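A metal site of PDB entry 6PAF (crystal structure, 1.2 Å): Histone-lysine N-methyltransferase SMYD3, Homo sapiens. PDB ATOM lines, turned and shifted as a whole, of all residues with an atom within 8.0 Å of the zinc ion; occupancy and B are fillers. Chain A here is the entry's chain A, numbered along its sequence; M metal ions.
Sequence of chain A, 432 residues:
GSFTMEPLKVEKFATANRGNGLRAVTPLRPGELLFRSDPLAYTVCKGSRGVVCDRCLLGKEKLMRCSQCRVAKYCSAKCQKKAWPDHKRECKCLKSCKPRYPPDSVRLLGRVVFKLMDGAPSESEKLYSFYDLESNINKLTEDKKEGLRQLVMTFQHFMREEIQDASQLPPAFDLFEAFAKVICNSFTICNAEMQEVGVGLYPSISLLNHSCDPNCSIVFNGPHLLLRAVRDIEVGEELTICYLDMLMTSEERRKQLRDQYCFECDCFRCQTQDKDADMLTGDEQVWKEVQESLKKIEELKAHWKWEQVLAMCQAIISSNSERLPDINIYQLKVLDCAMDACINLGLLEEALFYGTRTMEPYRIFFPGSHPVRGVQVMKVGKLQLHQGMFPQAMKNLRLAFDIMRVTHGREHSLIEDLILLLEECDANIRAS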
ATOM      1  N   ASP A  54     -10.395  37.175  23.081  1.00  0.00           N
ATOM      2  CA  ASP A  54     -10.332  35.855  22.437  1.00  0.00           C
ATOM      3  C   ASP A  54     -11.141  35.815  21.159  1.00  0.00           C
ATOM      4  O   ASP A  54     -10.780  35.108  20.223  1.00  0.00           O
ATOM      5  CB  ASP A  54     -10.998  34.818  23.332  1.00  0.00           C
ATOM      6  CG  ASP A  54     -10.034  34.029  24.156  1.00  0.00           C
ATOM      7  OD1 ASP A  54      -9.182  34.624  24.846  1.00  0.00           O
ATOM      8  OD2 ASP A  54     -10.142  32.794  24.137  1.00  0.00           O
ATOM      9  N   ARG A  65     -13.083  37.802  32.001  1.00  0.00           N
ATOM     10  CA  ARG A  65     -12.694  36.419  31.807  1.00  0.00           C
ATOM     11  C   ARG A  65     -13.902  35.483  31.896  1.00  0.00           C
ATOM     12  O   ARG A  65     -14.902  35.785  32.542  1.00  0.00           O
ATOM     13  CB  ARG A  65     -11.634  35.992  32.810  1.00  0.00           C
ATOM     14  CG  ARG A  65     -12.112  35.982  34.220  1.00  0.00           C
ATOM     15  CD  ARG A  65     -10.976  35.834  35.201  1.00  0.00           C
ATOM     16  NE  ARG A  65     -11.457  36.048  36.550  1.00  0.00           N
ATOM     17  CZ  ARG A  65     -10.747  35.826  37.644  1.00  0.00           C
ATOM     18  NH1 ARG A  65      -9.499  35.380  37.534  1.00  0.00           N
ATOM     19  NH2 ARG A  65     -11.280  36.043  38.838  1.00  0.00           N
ATOM     20  N   CYS A  66     -13.791  34.360  31.205  1.00  0.00           N
ATOM     21  CA  CYS A  66     -14.751  33.273  31.359  1.00  0.00           C
ATOM     22  C   CYS A  66     -14.688  32.767  32.779  1.00  0.00           C
ATOM     23  O   CYS A  66     -13.620  32.405  33.289  1.00  0.00           O
ATOM     24  CB  CYS A  66     -14.397  32.123  30.422  1.00  0.00           C
ATOM     25  SG  CYS A  66     -15.462  30.651  30.642  1.00  0.00           S
ATOM     26  N   SER A  67     -15.824  32.764  33.457  1.00  0.00           N
ATOM     27  CA  SER A  67     -15.770  32.381  34.838  1.00  0.00           C
ATOM     28  C   SER A  67     -15.425  30.906  35.000  1.00  0.00           C
ATOM     29  O   SER A  67     -14.870  30.523  36.038  1.00  0.00           O
ATOM     30  CB  SER A  67     -17.110  32.673  35.478  1.00  0.00           C
ATOM     31  OG  SER A  67     -17.017  32.246  36.796  1.00  0.00           O
ATOM     32  N   GLN A  68     -15.771  30.078  34.028  1.00  0.00           N
ATOM     33  CA  GLN A  68     -15.613  28.627  34.192  1.00  0.00           C
ATOM     34  C   GLN A  68     -14.140  28.230  34.085  1.00  0.00           C
ATOM     35  O   GLN A  68     -13.638  27.479  34.932  1.00  0.00           O
ATOM     36  CB  GLN A  68     -16.467  27.876  33.176  1.00  0.00           C
ATOM     37  N   CYS A  69     -13.447  28.713  33.059  1.00  0.00           N
ATOM     38  CA  CYS A  69     -12.051  28.363  32.880  1.00  0.00           C
ATOM     39  C   CYS A  69     -11.082  29.431  33.348  1.00  0.00           C
ATOM     40  O   CYS A  69      -9.944  29.102  33.728  1.00  0.00           O
ATOM     41  CB  CYS A  69     -11.766  28.038  31.400  1.00  0.00           C
ATOM     42  SG  CYS A  69     -11.939  29.354  30.251  1.00  0.00           S
ATOM     43  N   ARG A  70     -11.495  30.704  33.289  1.00  0.00           N
ATOM     44  CA  ARG A  70     -10.648  31.860  33.596  1.00  0.00           C
ATOM     45  C   ARG A  70      -9.433  31.972  32.684  1.00  0.00           C
ATOM     46  O   ARG A  70      -8.462  32.675  33.004  1.00  0.00           O
ATOM     47  CB  ARG A  70     -10.260  31.934  35.068  1.00  0.00           C
ATOM     48  CG  ARG A  70     -11.469  32.124  35.977  1.00  0.00           C
ATOM     49  CD  ARG A  70     -11.032  32.295  37.394  1.00  0.00           C
ATOM     50  NE  ARG A  70     -12.108  32.793  38.236  1.00  0.00           N
ATOM     51  CZ  ARG A  70     -11.991  32.920  39.551  1.00  0.00           C
ATOM     52  NH1 ARG A  70     -10.843  32.592  40.120  1.00  0.00           N
ATOM     53  NH2 ARG A  70     -13.001  33.399  40.278  1.00  0.00           N
ATOM     54  N   VAL A  71      -9.476  31.309  31.541  1.00  0.00           N
ATOM     55  CA  VAL A  71      -8.428  31.421  30.537  1.00  0.00           C
ATOM     56  C   VAL A  71      -8.882  32.301  29.385  1.00  0.00           C
ATOM     57  O   VAL A  71      -8.170  33.228  28.975  1.00  0.00           O
ATOM     58  CB  VAL A  71      -7.992  30.015  30.057  1.00  0.00           C
ATOM     59  CG1 VAL A  71      -6.945  30.130  28.972  1.00  0.00           C
ATOM     60  CG2 VAL A  71      -7.451  29.212  31.230  1.00  0.00           C
ATOM     61  N   ALA A  72     -10.053  32.002  28.846  1.00  0.00           N
ATOM     62  CA  ALA A  72     -10.586  32.821  27.759  1.00  0.00           C
ATOM     63  C   ALA A  72     -10.951  34.189  28.321  1.00  0.00           C
ATOM     64  O   ALA A  72     -11.540  34.295  29.405  1.00  0.00           O
ATOM     65  CB  ALA A  72     -11.831  32.156  27.166  1.00  0.00           C
ATOM     66  N   LYS A  73     -10.620  35.239  27.574  1.00  0.00           N
ATOM     67  CA  LYS A  73     -10.875  36.592  28.024  1.00  0.00           C
ATOM     68  C   LYS A  73     -11.476  37.398  26.875  1.00  0.00           C
ATOM     69  O   LYS A  73     -11.144  37.203  25.709  1.00  0.00           O
ATOM     70  CB  LYS A  73      -9.621  37.268  28.600  1.00  0.00           C
ATOM     71  CG  LYS A  73      -9.171  36.728  29.989  1.00  0.00           C
ATOM     72  CD  LYS A  73      -8.038  37.606  30.553  1.00  0.00           C
ATOM     73  CE  LYS A  73      -7.607  37.224  31.959  1.00  0.00           C
ATOM     74  NZ  LYS A  73      -7.016  35.867  32.016  1.00  0.00           N
ATOM     75  N   TYR A  74     -12.363  38.327  27.232  1.00  0.00           N
ATOM     76  CA  TYR A  74     -13.193  38.956  26.226  1.00  0.00           C
ATOM     77  C   TYR A  74     -13.312  40.462  26.456  1.00  0.00           C
ATOM     78  O   TYR A  74     -13.252  40.935  27.590  1.00  0.00           O
ATOM     79  CB  TYR A  74     -14.580  38.321  26.211  1.00  0.00           C
ATOM     80  CG  TYR A  74     -14.558  36.836  25.986  1.00  0.00           C
ATOM     81  CD1 TYR A  74     -14.364  36.312  24.712  1.00  0.00           C
ATOM     82  CD2 TYR A  74     -14.699  35.968  27.051  1.00  0.00           C
ATOM     83  CE1 TYR A  74     -14.352  34.948  24.471  1.00  0.00           C
ATOM     84  CE2 TYR A  74     -14.700  34.591  26.836  1.00  0.00           C
ATOM     85  CZ  TYR A  74     -14.500  34.109  25.546  1.00  0.00           C
ATOM     86  OH  TYR A  74     -14.511  32.741  25.327  1.00  0.00           O
ATOM     87  N   GLN A  80     -18.021  37.566  24.691  1.00  0.00           N
ATOM     88  CA  GLN A  80     -17.952  36.366  25.542  1.00  0.00           C
ATOM     89  C   GLN A  80     -19.092  35.426  25.221  1.00  0.00           C
ATOM     90  O   GLN A  80     -18.891  34.203  25.098  1.00  0.00           O
ATOM     91  CB  GLN A  80     -17.966  36.715  27.025  1.00  0.00           C
ATOM     92  CG  GLN A  80     -17.968  35.475  27.924  1.00  0.00           C
ATOM     93  CD  GLN A  80     -17.781  35.803  29.379  1.00  0.00           C
ATOM     94  OE1 GLN A  80     -17.506  36.957  29.724  1.00  0.00           O
ATOM     95  NE2 GLN A  80     -17.937  34.813  30.239  1.00  0.00           N
ATOM     96  N   TRP A  84     -19.156  31.610  23.151  1.00  0.00           N
ATOM     97  CA  TRP A  84     -19.438  30.430  23.969  1.00  0.00           C
ATOM     98  C   TRP A  84     -19.573  29.150  23.162  1.00  0.00           C
ATOM     99  O   TRP A  84     -18.927  28.145  23.513  1.00  0.00           O
ATOM    100  CB  TRP A  84     -20.635  30.692  24.869  1.00  0.00           C
ATOM    101  CG  TRP A  84     -20.983  29.506  25.685  1.00  0.00           C
ATOM    102  CD1 TRP A  84     -22.133  28.765  25.607  1.00  0.00           C
ATOM    103  CD2 TRP A  84     -20.194  28.913  26.718  1.00  0.00           C
ATOM    104  NE1 TRP A  84     -22.098  27.748  26.537  1.00  0.00           N
ATOM    105  CE2 TRP A  84     -20.907  27.801  27.213  1.00  0.00           C
ATOM    106  CE3 TRP A  84     -18.921  29.192  27.243  1.00  0.00           C
ATOM    107  CZ2 TRP A  84     -20.427  26.999  28.249  1.00  0.00           C
ATOM    108  CZ3 TRP A  84     -18.440  28.381  28.256  1.00  0.00           C
ATOM    109  CH2 TRP A  84     -19.182  27.307  28.739  1.00  0.00           C
ATOM    110  N   HIS A  87     -16.278  27.893  22.374  1.00  0.00           N
ATOM    111  CA  HIS A  87     -15.412  27.803  23.544  1.00  0.00           C
ATOM    112  C   HIS A  87     -15.864  26.740  24.532  1.00  0.00           C
ATOM    113  O   HIS A  87     -15.065  26.298  25.367  1.00  0.00           O
ATOM    114  CB  HIS A  87     -15.380  29.178  24.258  1.00  0.00           C
ATOM    115  CG  HIS A  87     -14.674  29.147  25.563  1.00  0.00           C
ATOM    116  ND1 HIS A  87     -13.337  28.808  25.673  1.00  0.00           N
ATOM    117  CD2 HIS A  87     -15.108  29.389  26.826  1.00  0.00           C
ATOM    118  CE1 HIS A  87     -12.994  28.838  26.944  1.00  0.00           C
ATOM    119  NE2 HIS A  87     -14.038  29.193  27.663  1.00  0.00           N
ATOM    120  N   LYS A  88     -17.111  26.292  24.429  1.00  0.00           N
ATOM    121  CA  LYS A  88     -17.732  25.482  25.486  1.00  0.00           C
ATOM    122  C   LYS A  88     -16.934  24.202  25.780  1.00  0.00           C
ATOM    123  O   LYS A  88     -16.723  23.843  26.940  1.00  0.00           O
ATOM    124  CB  LYS A  88     -19.170  25.134  25.058  1.00  0.00           C
ATOM    125  CG  LYS A  88     -19.844  24.042  25.829  1.00  0.00           C
ATOM    126  CD  LYS A  88     -21.249  23.753  25.276  1.00  0.00           C
ATOM    127  N   ARG A  89     -16.523  23.485  24.734  1.00  0.00           N
ATOM    128  CA  ARG A  89     -15.848  22.218  24.960  1.00  0.00           C
ATOM    129  C   ARG A  89     -14.406  22.416  25.376  1.00  0.00           C
ATOM    130  O   ARG A  89     -13.916  21.722  26.279  1.00  0.00           O
ATOM    131  CB  ARG A  89     -15.982  21.300  23.742  1.00  0.00           C
ATOM    132  CG  ARG A  89     -17.433  20.912  23.486  1.00  0.00           C
ATOM    133  CD  ARG A  89     -17.551  19.921  22.349  1.00  0.00           C
ATOM    134  NE  ARG A  89     -17.020  18.623  22.734  1.00  0.00           N
ATOM    135  CZ  ARG A  89     -16.822  17.606  21.896  1.00  0.00           C
ATOM    136  NH1 ARG A  89     -17.082  17.776  20.599  1.00  0.00           N
ATOM    137  NH2 ARG A  89     -16.276  16.478  22.317  1.00  0.00           N
ATOM    138  N   GLU A  90     -13.713  23.390  24.788  1.00  0.00           N
ATOM    139  CA  GLU A  90     -12.344  23.641  25.226  1.00  0.00           C
ATOM    140  C   GLU A  90     -12.310  24.199  26.642  1.00  0.00           C
ATOM    141  O   GLU A  90     -11.320  24.011  27.354  1.00  0.00           O
ATOM    142  CB  GLU A  90     -11.583  24.560  24.257  1.00  0.00           C
ATOM    143  CG  GLU A  90     -12.033  25.984  24.330  1.00  0.00           C
ATOM    144  CD  GLU A  90     -11.079  26.983  23.705  1.00  0.00           C
ATOM    145  OE1 GLU A  90     -10.057  26.673  23.059  1.00  0.00           O
ATOM    146  OE2 GLU A  90     -11.423  28.182  23.838  1.00  0.00           O
ATOM    147  N   CYS A  91     -13.397  24.845  27.078  1.00  0.00           N
ATOM    148  CA  CYS A  91     -13.427  25.422  28.402  1.00  0.00           C
ATOM    149  C   CYS A  91     -13.195  24.356  29.459  1.00  0.00           C
ATOM    150  O   CYS A  91     -12.384  24.515  30.371  1.00  0.00           O
ATOM    151  CB  CYS A  91     -14.805  26.074  28.598  1.00  0.00           C
ATOM    152  SG  CYS A  91     -15.015  26.934  30.171  1.00  0.00           S
ATOM    153  N   LYS A  92     -13.900  23.225  29.325  1.00  0.00           N
ATOM    154  CA  LYS A  92     -13.750  22.155  30.303  1.00  0.00           C
ATOM    155  C   LYS A  92     -12.342  21.577  30.291  1.00  0.00           C
ATOM    156  O   LYS A  92     -11.860  21.108  31.327  1.00  0.00           O
ATOM    157  CB  LYS A  92     -14.798  21.070  30.041  1.00  0.00           C
ATOM    158  N   CYS A  93     -11.669  21.632  29.143  1.00  0.00           N
ATOM    159  CA  CYS A  93     -10.303  21.114  29.057  1.00  0.00           C
ATOM    160  C   CYS A  93      -9.301  22.089  29.661  1.00  0.00           C
ATOM    161  O   CYS A  93      -8.421  21.677  30.429  1.00  0.00           O
ATOM    162  CB  CYS A  93      -9.958  20.863  27.606  1.00  0.00           C
ATOM    163  SG  CYS A  93     -11.030  19.662  26.782  1.00  0.00           S
ATOM    164  N   LEU A  94      -9.434  23.379  29.346  1.00  0.00           N
ATOM    165  CA  LEU A  94      -8.551  24.395  29.911  1.00  0.00           C
ATOM    166  C   LEU A  94      -8.668  24.421  31.431  1.00  0.00           C
ATOM    167  O   LEU A  94      -7.661  24.547  32.139  1.00  0.00           O
ATOM    168  CB  LEU A  94      -8.888  25.760  29.318  1.00  0.00           C
ATOM    169  CG  LEU A  94      -8.646  25.945  27.818  1.00  0.00           C
ATOM    170  CD1 LEU A  94      -9.385  27.152  27.263  1.00  0.00           C
ATOM    171  CD2 LEU A  94      -7.146  26.090  27.561  1.00  0.00           C
ATOM    172  N   LYS A  95      -9.899  24.297  31.942  1.00  0.00           N
ATOM    173  CA  LYS A  95     -10.105  24.189  33.389  1.00  0.00           C
ATOM    174  C   LYS A  95      -9.361  22.982  33.936  1.00  0.00           C
ATOM    175  O   LYS A  95      -8.575  23.096  34.898  1.00  0.00           O
ATOM    176  CB  LYS A  95     -11.597  24.082  33.689  1.00  0.00           C
ATOM    177  N   ARG A 107      -4.205  24.125  21.209  1.00  0.00           N
ATOM    178  CA  ARG A 107      -5.488  24.776  21.399  1.00  0.00           C
ATOM    179  C   ARG A 107      -6.182  24.940  20.057  1.00  0.00           C
ATOM    180  O   ARG A 107      -7.398  24.728  19.936  1.00  0.00           O
ATOM    181  CB  ARG A 107      -5.310  26.124  22.123  1.00  0.00           C
ATOM    182  CG  ARG A 107      -6.643  26.742  22.489  1.00  0.00           C
ATOM    183  CD  ARG A 107      -6.478  27.940  23.374  1.00  0.00           C
ATOM    184  NE  ARG A 107      -7.798  28.469  23.727  1.00  0.00           N
ATOM    185  CZ  ARG A 107      -8.003  29.650  24.291  1.00  0.00           C
ATOM    186  NH1 ARG A 107      -6.965  30.431  24.586  1.00  0.00           N
ATOM    187  NH2 ARG A 107      -9.240  30.067  24.610  1.00  0.00           N
HETATM  188 ZN    ZN M   1     -14.140  29.025  29.689  1.00  0.00          ZN
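A ring nitrogen (ND1) of His 87 is in hydrogen-bond range of the side-chain carboxylate of Glu 90. SG of Cys 69 lies close to N of Ala 72, 3.5 Å away. The side-chain sulfur of Cys 66 lies close to the backbone NH of Gln 68. O of Ala 72 lies within hydrogen-bond range of N of Cys 66 (2.9 Å). The side-chain sulfur (SG) of Cys 69 lies close to the backbone NH (N) of Val 71, 3.4 Å away.
Within 4 Å of the zinc ion: Cys 66, Cys 69, His 87 and Cys 91.
The zinc ion is bound by NE2 of His 87 (2.0 Å), SG of Cys 69 (2.3 Å), SG of Cys 66 (2.3 Å) and SG of Cys 91 (2.3 Å).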
